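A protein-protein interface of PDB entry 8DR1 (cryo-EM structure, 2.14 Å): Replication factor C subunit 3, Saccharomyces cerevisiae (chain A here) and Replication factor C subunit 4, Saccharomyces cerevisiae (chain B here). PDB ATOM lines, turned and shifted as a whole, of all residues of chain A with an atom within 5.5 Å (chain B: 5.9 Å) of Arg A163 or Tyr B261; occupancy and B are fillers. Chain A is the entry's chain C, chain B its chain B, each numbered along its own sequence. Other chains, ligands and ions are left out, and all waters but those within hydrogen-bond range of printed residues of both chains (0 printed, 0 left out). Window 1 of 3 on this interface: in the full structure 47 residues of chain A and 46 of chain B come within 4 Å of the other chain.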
ATOM      1  N   LEU A  50      21.110  -6.302  29.918  1.00  0.00           N
ATOM      2  CA  LEU A  50      21.934  -7.475  30.197  1.00  0.00           C
ATOM      3  C   LEU A  50      23.030  -7.541  29.141  1.00  0.00           C
ATOM      4  O   LEU A  50      22.767  -7.895  27.989  1.00  0.00           O
ATOM      5  CB  LEU A  50      21.092  -8.756  30.217  1.00  0.00           C
ATOM      6  CG  LEU A  50      21.801 -10.109  30.389  1.00  0.00           C
ATOM      7  CD1 LEU A  50      22.301 -10.669  29.073  1.00  0.00           C
ATOM      8  CD2 LEU A  50      22.955  -9.983  31.372  1.00  0.00           C
ATOM      9  N   TYR A  52      26.008  -9.497  27.828  1.00  0.00           N
ATOM     10  CA  TYR A  52      26.560 -10.846  27.876  1.00  0.00           C
ATOM     11  C   TYR A  52      27.698 -10.957  26.873  1.00  0.00           C
ATOM     12  O   TYR A  52      27.536 -10.584  25.708  1.00  0.00           O
ATOM     13  CB  TYR A  52      25.484 -11.891  27.568  1.00  0.00           C
ATOM     14  CG  TYR A  52      26.030 -13.282  27.336  1.00  0.00           C
ATOM     15  CD1 TYR A  52      26.470 -14.061  28.398  1.00  0.00           C
ATOM     16  CD2 TYR A  52      26.114 -13.813  26.056  1.00  0.00           C
ATOM     17  CE1 TYR A  52      26.970 -15.332  28.191  1.00  0.00           C
ATOM     18  CE2 TYR A  52      26.614 -15.083  25.840  1.00  0.00           C
ATOM     19  CZ  TYR A  52      27.041 -15.838  26.911  1.00  0.00           C
ATOM     20  OH  TYR A  52      27.540 -17.103  26.703  1.00  0.00           O
ATOM     21  N   CYS A 161      14.979  -8.563  31.354  1.00  0.00           N
ATOM     22  CA  CYS A 161      16.094  -7.784  30.834  1.00  0.00           C
ATOM     23  C   CYS A 161      16.126  -7.823  29.312  1.00  0.00           C
ATOM     24  O   CYS A 161      15.710  -8.802  28.687  1.00  0.00           O
ATOM     25  CB  CYS A 161      17.429  -8.303  31.384  1.00  0.00           C
ATOM     26  SG  CYS A 161      17.752  -7.863  33.107  1.00  0.00           S
ATOM     27  N   THR A 162      16.628  -6.739  28.724  1.00  0.00           N
ATOM     28  CA  THR A 162      16.906  -6.665  27.295  1.00  0.00           C
ATOM     29  C   THR A 162      18.369  -7.027  27.072  1.00  0.00           C
ATOM     30  O   THR A 162      19.258  -6.446  27.701  1.00  0.00           O
ATOM     31  CB  THR A 162      16.611  -5.267  26.747  1.00  0.00           C
ATOM     32  OG1 THR A 162      15.241  -4.930  26.998  1.00  0.00           O
ATOM     33  CG2 THR A 162      16.878  -5.207  25.248  1.00  0.00           C
ATOM     34  N   ARG A 163      18.613  -7.981  26.177  1.00  0.00           N
ATOM     35  CA  ARG A 163      19.912  -8.631  26.051  1.00  0.00           C
ATOM     36  C   ARG A 163      20.730  -8.006  24.929  1.00  0.00           C
ATOM     37  O   ARG A 163      20.228  -7.820  23.815  1.00  0.00           O
ATOM     38  CB  ARG A 163      19.732 -10.130  25.799  1.00  0.00           C
ATOM     39  CG  ARG A 163      21.029 -10.907  25.608  1.00  0.00           C
ATOM     40  CD  ARG A 163      20.748 -12.394  25.427  1.00  0.00           C
ATOM     41  NE  ARG A 163      21.951 -13.162  25.126  1.00  0.00           N
ATOM     42  CZ  ARG A 163      22.452 -13.337  23.910  1.00  0.00           C
ATOM     43  NH1 ARG A 163      21.876 -12.813  22.840  1.00  0.00           N
ATOM     44  NH2 ARG A 163      23.560 -14.059  23.763  1.00  0.00           N
ATOM     45  N   PHE A 164      21.989  -7.691  25.228  1.00  0.00           N
ATOM     46  CA  PHE A 164      22.967  -7.261  24.240  1.00  0.00           C
ATOM     47  C   PHE A 164      24.183  -8.171  24.332  1.00  0.00           C
ATOM     48  O   PHE A 164      24.747  -8.356  25.418  1.00  0.00           O
ATOM     49  CB  PHE A 164      23.384  -5.805  24.460  1.00  0.00           C
ATOM     50  CG  PHE A 164      22.285  -4.813  24.212  1.00  0.00           C
ATOM     51  CD1 PHE A 164      21.357  -4.529  25.199  1.00  0.00           C
ATOM     52  CD2 PHE A 164      22.180  -4.163  22.994  1.00  0.00           C
ATOM     53  CE1 PHE A 164      20.344  -3.616  24.975  1.00  0.00           C
ATOM     54  CE2 PHE A 164      21.169  -3.251  22.766  1.00  0.00           C
ATOM     55  CZ  PHE A 164      20.251  -2.977  23.758  1.00  0.00           C
ATOM     56  N   ARG A 165      24.590  -8.721  23.192  1.00  0.00           N
ATOM     57  CA  ARG A 165      25.715  -9.642  23.115  1.00  0.00           C
ATOM     58  C   ARG A 165      26.946  -8.910  22.597  1.00  0.00           C
ATOM     59  O   ARG A 165      26.901  -8.286  21.531  1.00  0.00           O
ATOM     60  CB  ARG A 165      25.382 -10.827  22.207  1.00  0.00           C
ATOM     61  CG  ARG A 165      26.091 -12.114  22.591  1.00  0.00           C
ATOM     62  CD  ARG A 165      25.942 -13.180  21.519  1.00  0.00           C
ATOM     63  NE  ARG A 165      26.866 -12.964  20.413  1.00  0.00           N
ATOM     64  CZ  ARG A 165      26.549 -12.387  19.260  1.00  0.00           C
ATOM     65  NH1 ARG A 165      25.318 -11.977  19.002  1.00  0.00           N
ATOM     66  NH2 ARG A 165      27.495 -12.218  18.341  1.00  0.00           N
ATOM     67  N   ILE B 227      17.429  -6.654  17.499  1.00  0.00           N
ATOM     68  CA  ILE B 227      17.241  -6.440  18.931  1.00  0.00           C
ATOM     69  C   ILE B 227      17.209  -7.760  19.693  1.00  0.00           C
ATOM     70  O   ILE B 227      17.810  -7.878  20.763  1.00  0.00           O
ATOM     71  CB  ILE B 227      15.962  -5.616  19.175  1.00  0.00           C
ATOM     72  CG1 ILE B 227      16.240  -4.135  18.907  1.00  0.00           C
ATOM     73  CG2 ILE B 227      15.448  -5.821  20.597  1.00  0.00           C
ATOM     74  CD1 ILE B 227      16.926  -3.418  20.054  1.00  0.00           C
ATOM     75  N   ASP B 229      18.170 -11.744  19.684  1.00  0.00           N
ATOM     76  CA  ASP B 229      19.025 -12.736  19.051  1.00  0.00           C
ATOM     77  C   ASP B 229      18.302 -14.075  18.972  1.00  0.00           C
ATOM     78  O   ASP B 229      17.508 -14.428  19.848  1.00  0.00           O
ATOM     79  CB  ASP B 229      20.332 -12.895  19.829  1.00  0.00           C
ATOM     80  CG  ASP B 229      21.557 -12.797  18.941  1.00  0.00           C
ATOM     81  OD1 ASP B 229      22.604 -12.321  19.424  1.00  0.00           O
ATOM     82  OD2 ASP B 229      21.475 -13.199  17.760  1.00  0.00           O
ATOM     83  N   SER B 230      18.584 -14.818  17.909  1.00  0.00           N
ATOM     84  CA  SER B 230      17.983 -16.134  17.754  1.00  0.00           C
ATOM     85  C   SER B 230      18.401 -17.019  18.926  1.00  0.00           C
ATOM     86  O   SER B 230      19.601 -17.121  19.216  1.00  0.00           O
ATOM     87  CB  SER B 230      18.410 -16.768  16.432  1.00  0.00           C
ATOM     88  OG  SER B 230      19.817 -16.727  16.275  1.00  0.00           O
ATOM     89  N   PRO B 231      17.465 -17.662  19.623  1.00  0.00           N
ATOM     90  CA  PRO B 231      17.849 -18.464  20.791  1.00  0.00           C
ATOM     91  C   PRO B 231      18.897 -19.504  20.424  1.00  0.00           C
ATOM     92  O   PRO B 231      18.756 -20.236  19.443  1.00  0.00           O
ATOM     93  CB  PRO B 231      16.531 -19.117  21.225  1.00  0.00           C
ATOM     94  CG  PRO B 231      15.459 -18.284  20.635  1.00  0.00           C
ATOM     95  CD  PRO B 231      16.012 -17.694  19.380  1.00  0.00           C
ATOM     96  N   HIS B 232      19.959 -19.565  21.225  1.00  0.00           N
ATOM     97  CA  HIS B 232      21.044 -20.498  20.953  1.00  0.00           C
ATOM     98  C   HIS B 232      20.634 -21.961  21.130  1.00  0.00           C
ATOM     99  O   HIS B 232      21.292 -22.833  20.549  1.00  0.00           O
ATOM    100  CB  HIS B 232      22.285 -20.164  21.797  1.00  0.00           C
ATOM    101  CG  HIS B 232      22.185 -20.547  23.241  1.00  0.00           C
ATOM    102  ND1 HIS B 232      21.223 -20.039  24.085  1.00  0.00           N
ATOM    103  CD2 HIS B 232      22.941 -21.383  23.992  1.00  0.00           C
ATOM    104  CE1 HIS B 232      21.384 -20.550  25.293  1.00  0.00           C
ATOM    105  NE2 HIS B 232      22.420 -21.369  25.263  1.00  0.00           N
ATOM    106  N   ILE B 235      20.110 -23.259  17.700  1.00  0.00           N
ATOM    107  CA  ILE B 235      21.377 -23.440  16.996  1.00  0.00           C
ATOM    108  C   ILE B 235      22.057 -24.720  17.461  1.00  0.00           C
ATOM    109  O   ILE B 235      22.618 -25.472  16.656  1.00  0.00           O
ATOM    110  CB  ILE B 235      22.283 -22.210  17.199  1.00  0.00           C
ATOM    111  CG1 ILE B 235      21.589 -20.945  16.687  1.00  0.00           C
ATOM    112  CG2 ILE B 235      23.618 -22.410  16.490  1.00  0.00           C
ATOM    113  CD1 ILE B 235      22.325 -19.663  17.018  1.00  0.00           C
ATOM    114  N   ASP B 255      28.443 -20.112  14.281  1.00  0.00           N
ATOM    115  CA  ASP B 255      27.232 -19.616  14.919  1.00  0.00           C
ATOM    116  C   ASP B 255      27.330 -19.535  16.435  1.00  0.00           C
ATOM    117  O   ASP B 255      26.530 -18.821  17.049  1.00  0.00           O
ATOM    118  CB  ASP B 255      26.039 -20.505  14.551  1.00  0.00           C
ATOM    119  CG  ASP B 255      25.682 -20.415  13.082  1.00  0.00           C
ATOM    120  OD1 ASP B 255      25.467 -19.286  12.593  1.00  0.00           O
ATOM    121  OD2 ASP B 255      25.619 -21.470  12.418  1.00  0.00           O
ATOM    122  N   LEU B 256      28.268 -20.250  17.054  1.00  0.00           N
ATOM    123  CA  LEU B 256      28.395 -20.249  18.506  1.00  0.00           C
ATOM    124  C   LEU B 256      29.738 -19.720  18.986  1.00  0.00           C
ATOM    125  O   LEU B 256      29.774 -18.783  19.791  1.00  0.00           O
ATOM    126  CB  LEU B 256      28.164 -21.668  19.045  1.00  0.00           C
ATOM    127  CG  LEU B 256      26.772 -22.236  18.759  1.00  0.00           C
ATOM    128  CD1 LEU B 256      26.727 -23.732  19.029  1.00  0.00           C
ATOM    129  CD2 LEU B 256      25.715 -21.509  19.578  1.00  0.00           C
ATOM    130  N   TRP B 257      30.848 -20.282  18.504  1.00  0.00           N
ATOM    131  CA  TRP B 257      32.150 -19.921  19.056  1.00  0.00           C
ATOM    132  C   TRP B 257      32.556 -18.512  18.642  1.00  0.00           C
ATOM    133  O   TRP B 257      33.039 -17.727  19.465  1.00  0.00           O
ATOM    134  CB  TRP B 257      33.208 -20.934  18.619  1.00  0.00           C
ATOM    135  CG  TRP B 257      34.503 -20.801  19.365  1.00  0.00           C
ATOM    136  CD1 TRP B 257      35.635 -20.169  18.936  1.00  0.00           C
ATOM    137  CD2 TRP B 257      34.803 -21.319  20.666  1.00  0.00           C
ATOM    138  NE1 TRP B 257      36.618 -20.258  19.892  1.00  0.00           N
ATOM    139  CE2 TRP B 257      36.132 -20.960  20.963  1.00  0.00           C
ATOM    140  CE3 TRP B 257      34.074 -22.050  21.610  1.00  0.00           C
ATOM    141  CZ2 TRP B 257      36.749 -21.308  22.163  1.00  0.00           C
ATOM    142  CZ3 TRP B 257      34.688 -22.394  22.800  1.00  0.00           C
ATOM    143  CH2 TRP B 257      36.012 -22.022  23.067  1.00  0.00           C
ATOM    144  N   LYS B 258      32.371 -18.173  17.366  1.00  0.00           N
ATOM    145  CA  LYS B 258      32.742 -16.843  16.900  1.00  0.00           C
ATOM    146  C   LYS B 258      31.810 -15.756  17.412  1.00  0.00           C
ATOM    147  O   LYS B 258      32.194 -14.583  17.391  1.00  0.00           O
ATOM    148  CB  LYS B 258      32.779 -16.802  15.373  1.00  0.00           C
ATOM    149  CG  LYS B 258      34.044 -17.408  14.786  1.00  0.00           C
ATOM    150  CD  LYS B 258      34.084 -17.523  13.250  1.00  0.00           C
ATOM    151  CE  LYS B 258      33.112 -16.633  12.465  1.00  0.00           C
ATOM    152  NZ  LYS B 258      33.150 -15.168  12.764  1.00  0.00           N
ATOM    153  N   LYS B 259      30.612 -16.107  17.876  1.00  0.00           N
ATOM    154  CA  LYS B 259      29.687 -15.117  18.410  1.00  0.00           C
ATOM    155  C   LYS B 259      29.941 -14.802  19.878  1.00  0.00           C
ATOM    156  O   LYS B 259      29.263 -13.930  20.432  1.00  0.00           O
ATOM    157  CB  LYS B 259      28.244 -15.599  18.236  1.00  0.00           C
ATOM    158  CG  LYS B 259      27.907 -16.083  16.831  1.00  0.00           C
ATOM    159  CD  LYS B 259      28.125 -15.001  15.772  1.00  0.00           C
ATOM    160  CE  LYS B 259      26.835 -14.604  15.059  1.00  0.00           C
ATOM    161  NZ  LYS B 259      25.975 -15.758  14.664  1.00  0.00           N
ATOM    162  N   GLY B 260      30.884 -15.485  20.518  1.00  0.00           N
ATOM    163  CA  GLY B 260      31.226 -15.216  21.898  1.00  0.00           C
ATOM    164  C   GLY B 260      30.536 -16.079  22.929  1.00  0.00           C
ATOM    165  O   GLY B 260      30.653 -15.791  24.125  1.00  0.00           O
ATOM    166  N   TYR B 261      29.819 -17.121  22.513  1.00  0.00           N
ATOM    167  CA  TYR B 261      29.181 -18.013  23.472  1.00  0.00           C
ATOM    168  C   TYR B 261      30.234 -18.848  24.189  1.00  0.00           C
ATOM    169  O   TYR B 261      31.121 -19.428  23.555  1.00  0.00           O
ATOM    170  CB  TYR B 261      28.169 -18.914  22.768  1.00  0.00           C
ATOM    171  CG  TYR B 261      26.898 -18.193  22.380  1.00  0.00           C
ATOM    172  CD1 TYR B 261      25.897 -17.962  23.313  1.00  0.00           C
ATOM    173  CD2 TYR B 261      26.703 -17.738  21.083  1.00  0.00           C
ATOM    174  CE1 TYR B 261      24.736 -17.300  22.967  1.00  0.00           C
ATOM    175  CE2 TYR B 261      25.544 -17.076  20.726  1.00  0.00           C
ATOM    176  CZ  TYR B 261      24.564 -16.859  21.673  1.00  0.00           C
ATOM    177  OH  TYR B 261      23.409 -16.202  21.323  1.00  0.00           O
ATOM    178  N   SER B 262      30.136 -18.906  25.513  1.00  0.00           N
ATOM    179  CA  SER B 262      31.114 -19.633  26.308  1.00  0.00           C
ATOM    180  C   SER B 262      30.956 -21.139  26.118  1.00  0.00           C
ATOM    181  O   SER B 262      29.872 -21.640  25.808  1.00  0.00           O
ATOM    182  CB  SER B 262      30.971 -19.273  27.787  1.00  0.00           C
ATOM    183  OG  SER B 262      29.735 -19.729  28.306  1.00  0.00           O
ATOM    184  N   SER B 263      32.061 -21.862  26.312  1.00  0.00           N
ATOM    185  CA  SER B 263      32.037 -23.312  26.147  1.00  0.00           C
ATOM    186  C   SER B 263      31.108 -23.970  27.162  1.00  0.00           C
ATOM    187  O   SER B 263      30.408 -24.936  26.837  1.00  0.00           O
ATOM    188  CB  SER B 263      33.453 -23.876  26.270  1.00  0.00           C
ATOM    189  OG  SER B 263      34.004 -23.608  27.547  1.00  0.00           O
ATOM    190  N   ASP B 265      28.393 -22.696  28.510  1.00  0.00           N
ATOM    191  CA  ASP B 265      27.027 -22.496  28.039  1.00  0.00           C
ATOM    192  C   ASP B 265      26.696 -23.457  26.905  1.00  0.00           C
ATOM    193  O   ASP B 265      25.611 -24.048  26.877  1.00  0.00           O
ATOM    194  CB  ASP B 265      26.834 -21.047  27.585  1.00  0.00           C
ATOM    195  CG  ASP B 265      26.637 -20.087  28.746  1.00  0.00           C
ATOM    196  OD1 ASP B 265      26.178 -20.528  29.820  1.00  0.00           O
ATOM    197  OD2 ASP B 265      26.936 -18.887  28.581  1.00  0.00           O
ATOM    198  N   ILE B 266      27.630 -23.635  25.967  1.00  0.00           N
ATOM    199  CA  ILE B 266      27.388 -24.518  24.828  1.00  0.00           C
ATOM    200  C   ILE B 266      27.154 -25.947  25.302  1.00  0.00           C
ATOM    201  O   ILE B 266      26.222 -26.621  24.853  1.00  0.00           O
ATOM    202  CB  ILE B 266      28.560 -24.439  23.832  1.00  0.00           C
ATOM    203  CG1 ILE B 266      28.584 -23.067  23.151  1.00  0.00           C
ATOM    204  CG2 ILE B 266      28.460 -25.555  22.794  1.00  0.00           C
ATOM    205  CD1 ILE B 266      29.857 -22.785  22.384  1.00  0.00           C
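Of the printed residues of chain B, Arg A163 touches Ile B227, Asp B229 and Tyr B261. Tyr B261 touches three residues of chain A. Of the printed residues of chain A, Lys B259 touches Arg A165 (2.6 Å). Of the printed residues of chain A, Asp B265 touches Tyr A52. Of the printed residues of chain A, Ser B262 touches Tyr A52 (3.4 Å). Asp B255 touches none of the printed residues of chain A. Pro B231 touches none of the printed residues of chain A. The nearest printed residue of chain B that does not touch Arg A163 is Ser B230 (6.1 Å).
The backbone carbonyl oxygen (O) of Leu B256 lies within hydrogen-bond range of the backbone NH (N) of Tyr B261. The side-chain hydroxyl of Ser B262 sits at hydrogen-bond distance from the side-chain carboxylate of Asp B265 (2.9 Å). The backbone NH (N) of Tyr A52 is in hydrogen-bond range of the backbone carbonyl oxygen (O) of Phe A164 (2.9 Å).
Hydrophobic or aromatic side chains of chain B that line the printed part of chain A: Tyr B261. Along chain B the printed residues that touch a printed residue of chain A span positions 227 to 265. Hydrophobic or aromatic side chains of chain A that line the printed part of chain B: Tyr A52. Among the printed residues, 9 pairs touch across the chains. Among the printed residues, Asp or Glu carboxylates within 4 Å of a Lys or Arg side-chain nitrogen of the other chain: Arg A163 with Asp B229 (3.5 Å) and Arg A165 with Asp B229 (2.8 Å).
Among the printed residues, pairs that only touch across the chains: Tyr A52 with Tyr B261, Arg A163 with Ile B227 and Arg A165 with Tyr B261.
The guanidinium group of Arg A163 lies within salt-bridge range of the side-chain carboxylate of Asp B229, 3.5 Å away. The side-chain carboxylate (OD1) of Asp B229 lies within salt-bridge range of the guanidinium group (NH1) of Arg A165. NE of Arg A165 sits at hydrogen-bond distance from O of Lys B259, at 2.6 Å. OH of Tyr B261 lies within hydrogen-bond range of NH2 of Arg A163 (3.3 Å). The side-chain hydroxyl (OH) of Tyr A52 lies within hydrogen-bond range of the backbone NH (N) of Ser B262, at 3.4 Å. The side-chain carboxylate of Asp B265 lies within hydrogen-bond range of the side-chain hydroxyl of Tyr A52 (2.7 Å).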
